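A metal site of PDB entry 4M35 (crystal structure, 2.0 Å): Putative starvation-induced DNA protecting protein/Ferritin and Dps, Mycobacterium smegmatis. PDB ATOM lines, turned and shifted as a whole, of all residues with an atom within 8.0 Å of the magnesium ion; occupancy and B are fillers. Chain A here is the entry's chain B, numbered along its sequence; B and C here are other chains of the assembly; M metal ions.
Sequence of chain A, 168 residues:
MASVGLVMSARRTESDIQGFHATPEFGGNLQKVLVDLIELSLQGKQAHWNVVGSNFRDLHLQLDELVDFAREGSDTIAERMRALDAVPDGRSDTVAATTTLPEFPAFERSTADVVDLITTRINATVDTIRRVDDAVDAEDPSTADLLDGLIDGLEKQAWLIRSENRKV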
ATOM      1  N   SER A  54     -16.763  22.308 -18.952  1.00  0.00           N
ATOM      2  CA  SER A  54     -15.719  21.909 -19.911  1.00  0.00           C
ATOM      3  C   SER A  54     -15.303  23.058 -20.805  1.00  0.00           C
ATOM      4  O   SER A  54     -16.121  23.687 -21.454  1.00  0.00           O
ATOM      5  CB  SER A  54     -16.226  20.740 -20.763  1.00  0.00           C
ATOM      6  OG  SER A  54     -16.825  19.746 -19.954  1.00  0.00           O
ATOM      7  N   ASN A  55     -13.989  23.301 -20.836  1.00  0.00           N
ATOM      8  CA  ASN A  55     -13.367  24.422 -21.545  1.00  0.00           C
ATOM      9  C   ASN A  55     -13.770  25.806 -21.020  1.00  0.00           C
ATOM     10  O   ASN A  55     -13.875  26.774 -21.778  1.00  0.00           O
ATOM     11  CB  ASN A  55     -13.580  24.330 -23.067  1.00  0.00           C
ATOM     12  CG  ASN A  55     -12.465  25.009 -23.832  1.00  0.00           C
ATOM     13  OD1 ASN A  55     -11.344  25.104 -23.338  1.00  0.00           O
ATOM     14  ND2 ASN A  55     -12.772  25.477 -25.028  1.00  0.00           N
ATOM     15  N   PHE A  56     -13.985  25.872 -19.719  1.00  0.00           N
ATOM     16  CA  PHE A  56     -14.245  27.130 -19.025  1.00  0.00           C
ATOM     17  C   PHE A  56     -13.259  28.227 -19.424  1.00  0.00           C
ATOM     18  O   PHE A  56     -13.674  29.305 -19.850  1.00  0.00           O
ATOM     19  CB  PHE A  56     -14.177  26.918 -17.502  1.00  0.00           C
ATOM     20  CG  PHE A  56     -13.951  28.186 -16.719  1.00  0.00           C
ATOM     21  CD1 PHE A  56     -14.991  29.086 -16.513  1.00  0.00           C
ATOM     22  CD2 PHE A  56     -12.697  28.472 -16.195  1.00  0.00           C
ATOM     23  CE1 PHE A  56     -14.779  30.260 -15.792  1.00  0.00           C
ATOM     24  CE2 PHE A  56     -12.480  29.638 -15.476  1.00  0.00           C
ATOM     25  CZ  PHE A  56     -13.520  30.538 -15.270  1.00  0.00           C
ATOM     26  N   ARG A  57     -11.972  27.951 -19.286  1.00  0.00           N
ATOM     27  CA  ARG A  57     -10.942  28.984 -19.381  1.00  0.00           C
ATOM     28  C   ARG A  57     -10.938  29.693 -20.727  1.00  0.00           C
ATOM     29  O   ARG A  57     -10.974  30.926 -20.782  1.00  0.00           O
ATOM     30  CB  ARG A  57      -9.564  28.416 -19.032  1.00  0.00           C
ATOM     31  CG  ARG A  57      -8.490  29.470 -18.873  1.00  0.00           C
ATOM     32  CD  ARG A  57      -7.160  28.852 -18.503  1.00  0.00           C
ATOM     33  NE  ARG A  57      -6.092  29.847 -18.420  1.00  0.00           N
ATOM     34  CZ  ARG A  57      -5.326  30.217 -19.438  1.00  0.00           C
ATOM     35  NH1 ARG A  57      -5.498  29.680 -20.648  1.00  0.00           N
ATOM     36  NH2 ARG A  57      -4.379  31.122 -19.256  1.00  0.00           N
ATOM     37  N   ASP A  58     -10.897  28.916 -21.822  1.00  0.00           N
ATOM     38  CA  ASP A  58     -10.954  29.476 -23.174  1.00  0.00           C
ATOM     39  C   ASP A  58     -12.141  30.417 -23.368  1.00  0.00           C
ATOM     40  O   ASP A  58     -11.988  31.491 -23.949  1.00  0.00           O
ATOM     41  CB  ASP A  58     -11.054  28.363 -24.220  1.00  0.00           C
ATOM     42  CG  ASP A  58      -9.694  27.960 -24.769  1.00  0.00           C
ATOM     43  OD1 ASP A  58      -8.798  28.820 -24.921  1.00  0.00           O
ATOM     44  OD2 ASP A  58      -9.536  26.766 -25.072  1.00  0.00           O
ATOM     45  N   LEU A  59     -13.317  30.019 -22.894  1.00  0.00           N
ATOM     46  CA  LEU A  59     -14.520  30.830 -23.044  1.00  0.00           C
ATOM     47  C   LEU A  59     -14.472  32.066 -22.158  1.00  0.00           C
ATOM     48  O   LEU A  59     -14.769  33.167 -22.609  1.00  0.00           O
ATOM     49  CB  LEU A  59     -15.793  30.012 -22.777  1.00  0.00           C
ATOM     50  CG  LEU A  59     -16.505  29.411 -23.997  1.00  0.00           C
ATOM     51  CD1 LEU A  59     -16.948  30.509 -24.975  1.00  0.00           C
ATOM     52  CD2 LEU A  59     -15.653  28.364 -24.696  1.00  0.00           C
ATOM     53  N   LEU A  61     -11.823  33.595 -21.256  1.00  0.00           N
ATOM     54  CA  LEU A  61     -10.881  34.524 -21.905  1.00  0.00           C
ATOM     55  C   LEU A  61     -11.421  35.152 -23.197  1.00  0.00           C
ATOM     56  O   LEU A  61     -11.234  36.351 -23.419  1.00  0.00           O
ATOM     57  CB  LEU A  61      -9.540  33.826 -22.176  1.00  0.00           C
ATOM     58  CG  LEU A  61      -8.717  33.436 -20.950  1.00  0.00           C
ATOM     59  CD1 LEU A  61      -7.599  32.482 -21.337  1.00  0.00           C
ATOM     60  CD2 LEU A  61      -8.173  34.684 -20.224  1.00  0.00           C
ATOM     61  N   GLU A 164     -16.621  26.234 -30.889  1.00  0.00           N
ATOM     62  CA  GLU A 164     -16.599  25.299 -29.762  1.00  0.00           C
ATOM     63  C   GLU A 164     -17.723  24.258 -29.800  1.00  0.00           C
ATOM     64  O   GLU A 164     -17.508  23.088 -29.446  1.00  0.00           O
ATOM     65  CB  GLU A 164     -16.624  26.070 -28.432  1.00  0.00           C
ATOM     66  CG  GLU A 164     -16.895  25.251 -27.166  1.00  0.00           C
ATOM     67  CD  GLU A 164     -15.722  24.384 -26.745  1.00  0.00           C
ATOM     68  OE1 GLU A 164     -15.963  23.336 -26.106  1.00  0.00           O
ATOM     69  OE2 GLU A 164     -14.560  24.732 -27.039  1.00  0.00           O
ATOM     70  N   SER B  54      -8.289  15.983 -22.190  1.00  0.00           N
ATOM     71  CA  SER B  54      -9.227  17.003 -22.650  1.00  0.00           C
ATOM     72  C   SER B  54      -8.965  18.374 -22.004  1.00  0.00           C
ATOM     73  O   SER B  54      -8.902  18.496 -20.789  1.00  0.00           O
ATOM     74  CB  SER B  54     -10.667  16.548 -22.376  1.00  0.00           C
ATOM     75  OG  SER B  54     -11.607  17.445 -22.948  1.00  0.00           O
ATOM     76  N   ASN B  55      -8.795  19.386 -22.855  1.00  0.00           N
ATOM     77  CA  ASN B  55      -8.478  20.748 -22.440  1.00  0.00           C
ATOM     78  C   ASN B  55      -7.133  20.865 -21.710  1.00  0.00           C
ATOM     79  O   ASN B  55      -6.982  21.643 -20.767  1.00  0.00           O
ATOM     80  CB  ASN B  55      -9.622  21.368 -21.623  1.00  0.00           C
ATOM     81  CG  ASN B  55      -9.604  22.889 -21.660  1.00  0.00           C
ATOM     82  OD1 ASN B  55      -9.161  23.479 -22.648  1.00  0.00           O
ATOM     83  ND2 ASN B  55     -10.066  23.527 -20.593  1.00  0.00           N
ATOM     84  N   PHE B  56      -6.159  20.075 -22.169  1.00  0.00           N
ATOM     85  CA  PHE B  56      -4.789  20.102 -21.669  1.00  0.00           C
ATOM     86  C   PHE B  56      -4.187  21.504 -21.626  1.00  0.00           C
ATOM     87  O   PHE B  56      -3.642  21.914 -20.595  1.00  0.00           O
ATOM     88  CB  PHE B  56      -3.883  19.200 -22.536  1.00  0.00           C
ATOM     89  CG  PHE B  56      -2.422  19.549 -22.438  1.00  0.00           C
ATOM     90  CD1 PHE B  56      -1.669  19.130 -21.344  1.00  0.00           C
ATOM     91  CD2 PHE B  56      -1.795  20.286 -23.433  1.00  0.00           C
ATOM     92  CE1 PHE B  56      -0.317  19.452 -21.232  1.00  0.00           C
ATOM     93  CE2 PHE B  56      -0.441  20.613 -23.342  1.00  0.00           C
ATOM     94  CZ  PHE B  56       0.301  20.198 -22.238  1.00  0.00           C
ATOM     95  N   ARG B  57      -4.284  22.227 -22.738  1.00  0.00           N
ATOM     96  CA  ARG B  57      -3.555  23.483 -22.916  1.00  0.00           C
ATOM     97  C   ARG B  57      -3.976  24.549 -21.897  1.00  0.00           C
ATOM     98  O   ARG B  57      -3.127  25.177 -21.265  1.00  0.00           O
ATOM     99  CB  ARG B  57      -3.688  24.008 -24.341  1.00  0.00           C
ATOM    100  CG  ARG B  57      -2.808  25.201 -24.666  1.00  0.00           C
ATOM    101  CD  ARG B  57      -2.991  25.647 -26.101  1.00  0.00           C
ATOM    102  NE  ARG B  57      -2.191  26.832 -26.409  1.00  0.00           N
ATOM    103  CZ  ARG B  57      -2.604  28.090 -26.270  1.00  0.00           C
ATOM    104  NH1 ARG B  57      -3.815  28.358 -25.822  1.00  0.00           N
ATOM    105  NH2 ARG B  57      -1.784  29.083 -26.590  1.00  0.00           N
ATOM    106  N   ASP B  58      -5.294  24.726 -21.738  1.00  0.00           N
ATOM    107  CA  ASP B  58      -5.851  25.664 -20.764  1.00  0.00           C
ATOM    108  C   ASP B  58      -5.345  25.412 -19.349  1.00  0.00           C
ATOM    109  O   ASP B  58      -4.953  26.347 -18.657  1.00  0.00           O
ATOM    110  CB  ASP B  58      -7.380  25.612 -20.751  1.00  0.00           C
ATOM    111  CG  ASP B  58      -8.020  26.686 -21.607  1.00  0.00           C
ATOM    112  OD1 ASP B  58      -7.511  27.827 -21.651  1.00  0.00           O
ATOM    113  OD2 ASP B  58      -9.062  26.388 -22.215  1.00  0.00           O
ATOM    114  N   LEU B  59      -5.356  24.148 -18.916  1.00  0.00           N
ATOM    115  CA  LEU B  59      -4.903  23.817 -17.575  1.00  0.00           C
ATOM    116  C   LEU B  59      -3.388  23.937 -17.442  1.00  0.00           C
ATOM    117  O   LEU B  59      -2.896  24.453 -16.442  1.00  0.00           O
ATOM    118  CB  LEU B  59      -5.412  22.438 -17.121  1.00  0.00           C
ATOM    119  CG  LEU B  59      -6.793  22.394 -16.436  1.00  0.00           C
ATOM    120  CD1 LEU B  59      -6.807  23.204 -15.142  1.00  0.00           C
ATOM    121  CD2 LEU B  59      -7.933  22.847 -17.362  1.00  0.00           C
ATOM    122  N   LEU B  61      -1.491  26.022 -19.060  1.00  0.00           N
ATOM    123  CA  LEU B  61      -1.231  27.466 -18.960  1.00  0.00           C
ATOM    124  C   LEU B  61      -1.661  28.074 -17.612  1.00  0.00           C
ATOM    125  O   LEU B  61      -0.898  28.808 -17.003  1.00  0.00           O
ATOM    126  CB  LEU B  61      -1.862  28.227 -20.133  1.00  0.00           C
ATOM    127  CG  LEU B  61      -1.304  27.898 -21.531  1.00  0.00           C
ATOM    128  CD1 LEU B  61      -2.242  28.379 -22.637  1.00  0.00           C
ATOM    129  CD2 LEU B  61       0.098  28.459 -21.738  1.00  0.00           C
ATOM    130  N   GLU B 164     -13.589  24.244 -14.568  1.00  0.00           N
ATOM    131  CA  GLU B 164     -13.516  23.233 -15.615  1.00  0.00           C
ATOM    132  C   GLU B 164     -14.373  21.989 -15.321  1.00  0.00           C
ATOM    133  O   GLU B 164     -14.992  21.428 -16.224  1.00  0.00           O
ATOM    134  CB  GLU B 164     -12.053  22.829 -15.853  1.00  0.00           C
ATOM    135  CG  GLU B 164     -11.814  21.585 -16.730  1.00  0.00           C
ATOM    136  CD  GLU B 164     -12.206  21.788 -18.189  1.00  0.00           C
ATOM    137  OE1 GLU B 164     -12.545  20.785 -18.854  1.00  0.00           O
ATOM    138  OE2 GLU B 164     -12.174  22.933 -18.679  1.00  0.00           O
ATOM    139  N   SER C  54     -14.932  20.764 -29.869  1.00  0.00           N
ATOM    140  CA  SER C  54     -14.511  20.803 -28.471  1.00  0.00           C
ATOM    141  C   SER C  54     -13.071  21.289 -28.292  1.00  0.00           C
ATOM    142  O   SER C  54     -12.147  20.727 -28.874  1.00  0.00           O
ATOM    143  CB  SER C  54     -14.695  19.425 -27.827  1.00  0.00           C
ATOM    144  OG  SER C  54     -14.183  19.405 -26.503  1.00  0.00           O
ATOM    145  N   ASN C  55     -12.908  22.322 -27.462  1.00  0.00           N
ATOM    146  CA  ASN C  55     -11.613  22.980 -27.223  1.00  0.00           C
ATOM    147  C   ASN C  55     -10.977  23.632 -28.466  1.00  0.00           C
ATOM    148  O   ASN C  55      -9.762  23.610 -28.641  1.00  0.00           O
ATOM    149  CB  ASN C  55     -10.614  22.042 -26.515  1.00  0.00           C
ATOM    150  CG  ASN C  55      -9.536  22.795 -25.763  1.00  0.00           C
ATOM    151  OD1 ASN C  55      -9.756  23.932 -25.335  1.00  0.00           O
ATOM    152  ND2 ASN C  55      -8.371  22.189 -25.603  1.00  0.00           N
ATOM    153  N   PHE C  56     -11.841  24.192 -29.321  1.00  0.00           N
ATOM    154  CA  PHE C  56     -11.433  24.917 -30.530  1.00  0.00           C
ATOM    155  C   PHE C  56     -10.348  25.967 -30.265  1.00  0.00           C
ATOM    156  O   PHE C  56      -9.306  25.965 -30.931  1.00  0.00           O
ATOM    157  CB  PHE C  56     -12.649  25.590 -31.190  1.00  0.00           C
ATOM    158  CG  PHE C  56     -12.298  26.707 -32.137  1.00  0.00           C
ATOM    159  CD1 PHE C  56     -12.368  28.035 -31.734  1.00  0.00           C
ATOM    160  CD2 PHE C  56     -11.885  26.432 -33.441  1.00  0.00           C
ATOM    161  CE1 PHE C  56     -12.031  29.077 -32.605  1.00  0.00           C
ATOM    162  CE2 PHE C  56     -11.549  27.462 -34.320  1.00  0.00           C
ATOM    163  CZ  PHE C  56     -11.629  28.793 -33.907  1.00  0.00           C
ATOM    164  N   ARG C  57     -10.602  26.854 -29.311  1.00  0.00           N
ATOM    165  CA  ARG C  57      -9.765  28.034 -29.105  1.00  0.00           C
ATOM    166  C   ARG C  57      -8.311  27.677 -28.771  1.00  0.00           C
ATOM    167  O   ARG C  57      -7.390  28.238 -29.365  1.00  0.00           O
ATOM    168  CB  ARG C  57     -10.370  28.971 -28.055  1.00  0.00           C
ATOM    169  CG  ARG C  57      -9.626  30.296 -27.904  1.00  0.00           C
ATOM    170  CD  ARG C  57     -10.281  31.160 -26.835  1.00  0.00           C
ATOM    171  NE  ARG C  57      -9.592  32.426 -26.632  1.00  0.00           N
ATOM    172  CZ  ARG C  57      -8.624  32.622 -25.741  1.00  0.00           C
ATOM    173  NH1 ARG C  57      -8.203  31.630 -24.968  1.00  0.00           N
ATOM    174  NH2 ARG C  57      -8.063  33.824 -25.631  1.00  0.00           N
ATOM    175  N   ASP C  58      -8.122  26.759 -27.824  1.00  0.00           N
ATOM    176  CA  ASP C  58      -6.779  26.285 -27.453  1.00  0.00           C
ATOM    177  C   ASP C  58      -6.003  25.776 -28.659  1.00  0.00           C
ATOM    178  O   ASP C  58      -4.839  26.124 -28.837  1.00  0.00           O
ATOM    179  CB  ASP C  58      -6.868  25.163 -26.418  1.00  0.00           C
ATOM    180  CG  ASP C  58      -6.674  25.643 -25.000  1.00  0.00           C
ATOM    181  OD1 ASP C  58      -5.896  26.592 -24.755  1.00  0.00           O
ATOM    182  OD2 ASP C  58      -7.316  25.054 -24.106  1.00  0.00           O
ATOM    183  N   LEU C  59      -6.652  24.955 -29.474  1.00  0.00           N
ATOM    184  CA  LEU C  59      -6.007  24.378 -30.650  1.00  0.00           C
ATOM    185  C   LEU C  59      -5.766  25.437 -31.716  1.00  0.00           C
ATOM    186  O   LEU C  59      -4.675  25.515 -32.269  1.00  0.00           O
ATOM    187  CB  LEU C  59      -6.817  23.212 -31.217  1.00  0.00           C
ATOM    188  CG  LEU C  59      -6.330  21.805 -30.854  1.00  0.00           C
ATOM    189  CD1 LEU C  59      -4.890  21.569 -31.313  1.00  0.00           C
ATOM    190  CD2 LEU C  59      -6.486  21.523 -29.353  1.00  0.00           C
ATOM    191  N   GLU C 164      -3.850  16.818 -25.846  1.00  0.00           N
ATOM    192  CA  GLU C 164      -5.311  16.974 -25.905  1.00  0.00           C
ATOM    193  C   GLU C 164      -6.056  15.637 -26.064  1.00  0.00           C
ATOM    194  O   GLU C 164      -7.089  15.420 -25.432  1.00  0.00           O
ATOM    195  CB  GLU C 164      -5.709  17.938 -27.026  1.00  0.00           C
ATOM    196  CG  GLU C 164      -7.209  17.997 -27.366  1.00  0.00           C
ATOM    197  CD  GLU C 164      -8.069  18.660 -26.282  1.00  0.00           C
ATOM    198  OE1 GLU C 164      -7.542  19.495 -25.512  1.00  0.00           O
ATOM    199  OE2 GLU C 164      -9.274  18.346 -26.209  1.00  0.00           O
HETATM  200 MG    MG M   1      -9.375  25.114 -23.764  1.00  0.00          MG
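Along chain A the residues within 4 Å of the magnesium ion span positions 55 to 58.
The nearest printed residue that does not touch the magnesium ion is Arg 57 of chain A (5.7 Å).
ND2 of Asn 55 of chain C sits at hydrogen-bond distance from OE1 of Glu 164 of chain C (2.8 Å).
The side-chain carboxylate of Glu 164 of chain A lies within hydrogen-bond range of the backbone NH of Asn 55 of chain C, 3.0 Å away.
NH1 of Arg 57 of chain B is in salt-bridge range of OD1 of Asp 58 of chain C (2.9 Å).
The backbone NH of Asn 55 of chain B sits at hydrogen-bond distance from the side-chain carboxylate of Glu 164 of chain C, 2.9 Å away.
OD1 of Asp 58 of chain A is in salt-bridge range of NH1 of Arg 57 of chain C, at 2.9 Å.
The backbone NH (N) of Asn 55 of chain A is in hydrogen-bond range of the side-chain carboxylate (OE2) of Glu 164 of chain B, at 2.8 Å.
The side-chain amide nitrogen (ND2) of Asn 55 of chain B is in hydrogen-bond range of the side-chain carboxylate (OE2) of Glu 164 of chain B (2.9 Å).
The side-chain carboxylate (OD1) of Asp 58 of chain B is in salt-bridge range of the guanidinium group (NH1) of Arg 57 of chain A (2.9 Å).
The magnesium ion is bound by OD1 of Asn 55 of chain B (2.0 Å), OD1 of Asn 55 of chain C (2.0 Å), OD1 of Asn 55 of chain A (2.0 Å), OD2 of Asp 58 of chain B (2.0 Å), OD2 of Asp 58 of chain C (2.1 Å) and OD2 of Asp 58 of chain A (2.1 Å).
The magnesium ion has six donor atoms within binding distance.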
